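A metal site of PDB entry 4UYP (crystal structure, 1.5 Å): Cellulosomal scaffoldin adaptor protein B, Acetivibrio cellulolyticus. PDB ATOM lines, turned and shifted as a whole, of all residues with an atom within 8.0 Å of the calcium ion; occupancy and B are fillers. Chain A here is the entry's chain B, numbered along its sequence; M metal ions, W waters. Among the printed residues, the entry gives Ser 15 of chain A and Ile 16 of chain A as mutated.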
ATOM      1  N   ILE A   3       2.164  12.693 -26.485  1.00  0.00           N
ATOM      2  CA  ILE A   3       2.477  12.828 -27.930  1.00  0.00           C
ATOM      3  C   ILE A   3       2.531  11.454 -28.576  1.00  0.00           C
ATOM      4  O   ILE A   3       3.173  10.562 -28.035  1.00  0.00           O
ATOM      5  CB  ILE A   3       3.865  13.499 -28.130  1.00  0.00           C
ATOM      6  CG1 ILE A   3       3.830  14.885 -27.444  1.00  0.00           C
ATOM      7  CG2 ILE A   3       4.363  13.504 -29.567  1.00  0.00           C
ATOM      8  CD1 ILE A   3       5.174  15.440 -27.058  1.00  0.00           C
ATOM      9  N   GLY A   5       3.620   8.455 -30.516  1.00  0.00           N
ATOM     10  CA  GLY A   5       5.031   8.097 -30.897  1.00  0.00           C
ATOM     11  C   GLY A   5       5.973   8.172 -29.731  1.00  0.00           C
ATOM     12  O   GLY A   5       7.027   7.559 -29.743  1.00  0.00           O
ATOM     13  N   ASP A   6       5.596   8.916 -28.672  1.00  0.00           N
ATOM     14  CA  ASP A   6       6.538   9.177 -27.590  1.00  0.00           C
ATOM     15  C   ASP A   6       6.396   8.186 -26.455  1.00  0.00           C
ATOM     16  O   ASP A   6       5.845   8.416 -25.399  1.00  0.00           O
ATOM     17  CB  ASP A   6       6.271  10.588 -26.998  1.00  0.00           C
ATOM     18  CG  ASP A   6       7.261  10.888 -25.925  1.00  0.00           C
ATOM     19  OD1 ASP A   6       8.352  10.325 -25.801  1.00  0.00           O
ATOM     20  OD2 ASP A   6       6.953  11.773 -25.075  1.00  0.00           O
ATOM     21  N   VAL A   7       6.863   6.949 -26.737  1.00  0.00           N
ATOM     22  CA  VAL A   7       6.485   5.809 -25.903  1.00  0.00           C
ATOM     23  C   VAL A   7       7.242   5.801 -24.547  1.00  0.00           C
ATOM     24  O   VAL A   7       6.730   5.228 -23.608  1.00  0.00           O
ATOM     25  CB  VAL A   7       6.657   4.469 -26.728  1.00  0.00           C
ATOM     26  CG1 VAL A   7       6.268   4.616 -28.224  1.00  0.00           C
ATOM     27  CG2 VAL A   7       8.050   4.077 -26.782  1.00  0.00           C
ATOM     28  N   ASP A   8       8.384   6.483 -24.487  1.00  0.00           N
ATOM     29  CA  ASP A   8       9.133   6.661 -23.226  1.00  0.00           C
ATOM     30  C   ASP A   8       8.729   7.914 -22.467  1.00  0.00           C
ATOM     31  O   ASP A   8       9.240   8.117 -21.364  1.00  0.00           O
ATOM     32  CB  ASP A   8      10.679   6.540 -23.357  1.00  0.00           C
ATOM     33  CG  ASP A   8      11.348   7.625 -24.198  1.00  0.00           C
ATOM     34  OD1 ASP A   8      10.612   8.651 -24.559  1.00  0.00           O
ATOM     35  OD2 ASP A   8      12.568   7.504 -24.433  1.00  0.00           O
ATOM     36  N   GLY A   9       7.813   8.704 -23.042  1.00  0.00           N
ATOM     37  CA  GLY A   9       7.238   9.881 -22.295  1.00  0.00           C
ATOM     38  C   GLY A   9       8.226  10.978 -22.114  1.00  0.00           C
ATOM     39  O   GLY A   9       8.036  11.764 -21.167  1.00  0.00           O
ATOM     40  N   ASN A  10       9.247  11.129 -22.894  1.00  0.00           N
ATOM     41  CA  ASN A  10      10.259  12.125 -22.624  1.00  0.00           C
ATOM     42  C   ASN A  10       9.926  13.457 -23.368  1.00  0.00           C
ATOM     43  O   ASN A  10      10.791  14.380 -23.309  1.00  0.00           O
ATOM     44  CB  ASN A  10      11.739  11.656 -22.887  1.00  0.00           C
ATOM     45  CG  ASN A  10      12.067  11.582 -24.388  1.00  0.00           C
ATOM     46  OD1 ASN A  10      11.163  11.511 -25.223  1.00  0.00           O
ATOM     47  ND2 ASN A  10      13.308  11.559 -24.708  1.00  0.00           N
ATOM     48  N   GLY A  11       8.795  13.505 -24.084  1.00  0.00           N
ATOM     49  CA  GLY A  11       8.449  14.769 -24.753  1.00  0.00           C
ATOM     50  C   GLY A  11       8.870  14.879 -26.212  1.00  0.00           C
ATOM     51  O   GLY A  11       8.638  15.943 -26.845  1.00  0.00           O
ATOM     52  N   SER A  12       9.536  13.826 -26.780  1.00  0.00           N
ATOM     53  CA  SER A  12      10.061  13.886 -28.085  1.00  0.00           C
ATOM     54  C   SER A  12       9.897  12.513 -28.751  1.00  0.00           C
ATOM     55  O   SER A  12      10.112  11.543 -28.035  1.00  0.00           O
ATOM     56  CB  SER A  12      11.533  14.109 -27.893  1.00  0.00           C
ATOM     57  OG  SER A  12      12.193  14.359 -29.079  1.00  0.00           O
ATOM     58  N   VAL A  13       9.584  12.459 -30.045  1.00  0.00           N
ATOM     59  CA  VAL A  13       9.558  11.179 -30.761  1.00  0.00           C
ATOM     60  C   VAL A  13      10.926  10.979 -31.380  1.00  0.00           C
ATOM     61  O   VAL A  13      11.422  11.757 -32.187  1.00  0.00           O
ATOM     62  CB  VAL A  13       8.483  11.222 -31.852  1.00  0.00           C
ATOM     63  CG1 VAL A  13       8.375   9.828 -32.464  1.00  0.00           C
ATOM     64  CG2 VAL A  13       7.129  11.573 -31.187  1.00  0.00           C
ATOM     65  N   ARG A  14      11.574   9.863 -30.975  1.00  0.00           N
ATOM     66  CA  ARG A  14      12.994   9.637 -31.252  1.00  0.00           C
ATOM     67  C   ARG A  14      13.179   8.194 -31.661  1.00  0.00           C
ATOM     68  O   ARG A  14      12.333   7.361 -31.440  1.00  0.00           O
ATOM     69  CB  ARG A  14      13.851   9.852 -30.004  1.00  0.00           C
ATOM     70  CG  ARG A  14      13.607  11.196 -29.334  1.00  0.00           C
ATOM     71  CD  ARG A  14      14.098  12.214 -30.350  1.00  0.00           C
ATOM     72  NE  ARG A  14      15.502  12.484 -30.328  1.00  0.00           N
ATOM     73  CZ  ARG A  14      16.225  13.076 -29.314  1.00  0.00           C
ATOM     74  NH1 ARG A  14      15.591  13.498 -28.203  1.00  0.00           N
ATOM     75  NH2 ARG A  14      17.582  13.248 -29.402  1.00  0.00           N
ATOM     76  N   SER A  15      14.359   7.924 -32.178  1.00  0.00           N
ATOM     77  CA  SER A  15      14.665   6.525 -32.633  1.00  0.00           C
ATOM     78  C   SER A  15      14.368   5.486 -31.592  1.00  0.00           C
ATOM     79  O   SER A  15      13.874   4.340 -31.857  1.00  0.00           O
ATOM     80  CB  SER A  15      16.092   6.400 -33.102  1.00  0.00           C
ATOM     81  OG  SER A  15      16.280   7.176 -34.287  1.00  0.00           O
ATOM     82  N   ILE A  16      14.767   5.815 -30.341  1.00  0.00           N
ATOM     83  CA  ILE A  16      14.627   4.819 -29.267  1.00  0.00           C
ATOM     84  C   ILE A  16      13.179   4.444 -29.014  1.00  0.00           C
ATOM     85  O   ILE A  16      12.878   3.339 -28.587  1.00  0.00           O
ATOM     86  CB  ILE A  16      15.351   5.276 -27.986  1.00  0.00           C
ATOM     87  CG1 ILE A  16      15.640   4.110 -27.006  1.00  0.00           C
ATOM     88  CG2 ILE A  16      14.560   6.386 -27.279  1.00  0.00           C
ATOM     89  CD1 ILE A  16      16.684   3.089 -27.549  1.00  0.00           C
ATOM     90  N   ASP A  17      12.226   5.402 -29.246  1.00  0.00           N
ATOM     91  CA  ASP A  17      10.808   5.060 -29.075  1.00  0.00           C
ATOM     92  C   ASP A  17      10.421   3.863 -29.939  1.00  0.00           C
ATOM     93  O   ASP A  17       9.648   3.043 -29.493  1.00  0.00           O
ATOM     94  CB  ASP A  17       9.927   6.321 -29.370  1.00  0.00           C
ATOM     95  CG  ASP A  17      10.089   7.444 -28.323  1.00  0.00           C
ATOM     96  OD1 ASP A  17       9.870   7.237 -27.099  1.00  0.00           O
ATOM     97  OD2 ASP A  17      10.392   8.602 -28.736  1.00  0.00           O
ATOM     98  N   ALA A  18      10.939   3.801 -31.171  1.00  0.00           N
ATOM     99  CA  ALA A  18      10.532   2.688 -32.044  1.00  0.00           C
ATOM    100  C   ALA A  18      11.202   1.416 -31.532  1.00  0.00           C
ATOM    101  O   ALA A  18      10.640   0.335 -31.720  1.00  0.00           O
ATOM    102  CB  ALA A  18      10.997   3.001 -33.503  1.00  0.00           C
ATOM    103  N   LEU A  20      11.673   0.677 -28.390  1.00  0.00           N
ATOM    104  CA  LEU A  20      10.849   0.239 -27.294  1.00  0.00           C
ATOM    105  C   LEU A  20       9.606  -0.459 -27.739  1.00  0.00           C
ATOM    106  O   LEU A  20       9.188  -1.484 -27.159  1.00  0.00           O
ATOM    107  CB  LEU A  20      10.476   1.383 -26.368  1.00  0.00           C
ATOM    108  CG  LEU A  20      11.699   1.975 -25.688  1.00  0.00           C
ATOM    109  CD1 LEU A  20      11.339   3.284 -24.933  1.00  0.00           C
ATOM    110  CD2 LEU A  20      12.117   0.985 -24.564  1.00  0.00           C
ATOM    111  N   TYR A  34       6.029   4.479 -19.124  1.00  0.00           N
ATOM    112  CA  TYR A  34       5.449   5.806 -19.222  1.00  0.00           C
ATOM    113  C   TYR A  34       4.015   5.501 -19.086  1.00  0.00           C
ATOM    114  O   TYR A  34       3.483   4.522 -19.634  1.00  0.00           O
ATOM    115  CB  TYR A  34       5.685   6.337 -20.606  1.00  0.00           C
ATOM    116  CG  TYR A  34       4.974   7.592 -20.968  1.00  0.00           C
ATOM    117  CD1 TYR A  34       4.707   8.600 -20.018  1.00  0.00           C
ATOM    118  CD2 TYR A  34       4.563   7.820 -22.312  1.00  0.00           C
ATOM    119  CE1 TYR A  34       4.067   9.742 -20.399  1.00  0.00           C
ATOM    120  CE2 TYR A  34       3.958   8.998 -22.701  1.00  0.00           C
ATOM    121  CZ  TYR A  34       3.726   9.952 -21.731  1.00  0.00           C
ATOM    122  OH  TYR A  34       3.173  11.127 -22.188  1.00  0.00           O
ATOM    123  N   VAL A  57       6.768   4.555 -36.226  1.00  0.00           N
ATOM    124  CA  VAL A  57       7.534   5.516 -35.459  1.00  0.00           C
ATOM    125  C   VAL A  57       8.920   5.743 -36.039  1.00  0.00           C
ATOM    126  O   VAL A  57       9.388   6.898 -36.161  1.00  0.00           O
ATOM    127  CB  VAL A  57       7.583   5.092 -33.946  1.00  0.00           C
ATOM    128  CG1 VAL A  57       8.482   6.017 -33.133  1.00  0.00           C
ATOM    129  CG2 VAL A  57       6.165   5.146 -33.400  1.00  0.00           C
HETATM  130 CA    CA M   1      10.455   9.692 -26.618  1.00  0.00          CA
HETATM  131  O   HOH W   1      12.781   9.059 -26.640  1.00  0.00           O
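The calcium ion is bound by OD1 of Asp 8, 2.3 Å away.
The calcium ion is bound by the side-chain carboxylate (OD1) of Asp 6 (2.3 Å).
O of Ser 12 is bound to the calcium ion, 2.4 Å away.
OD2 of Asp 17 binds the calcium ion (2.4 Å).
The calcium ion is bound by OD1 of Asn 10.
Water W1 binds the calcium ion (2.4 Å).
OD1 of Asp 17 binds the calcium ion, 2.6 Å away.
The calcium ion has seven donor atoms within binding distance.
The backbone NH (N) of Gly 9 lies close to the side-chain carboxylate (OD1) of Asp 6 (3.2 Å).
The backbone NH (N) of Val 7 lies close to the side-chain carboxylate (OD1) of Asp 17.
N of Arg 14 lies close to OD2 of Asp 17, at 2.8 Å.
N of Gly 11 is in hydrogen-bond range of OD2 of Asp 6, at 2.7 Å.
Five residues have an atom within 4 Å of the calcium ion: Asp 6, Asp 8, Asn 10, Ser 12 and Asp 17.
Water W1 bridges the side-chain carboxylate of Asp 8 (2.7 Å) and the side-chain amide nitrogen of Asn 10 (3.2 Å).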
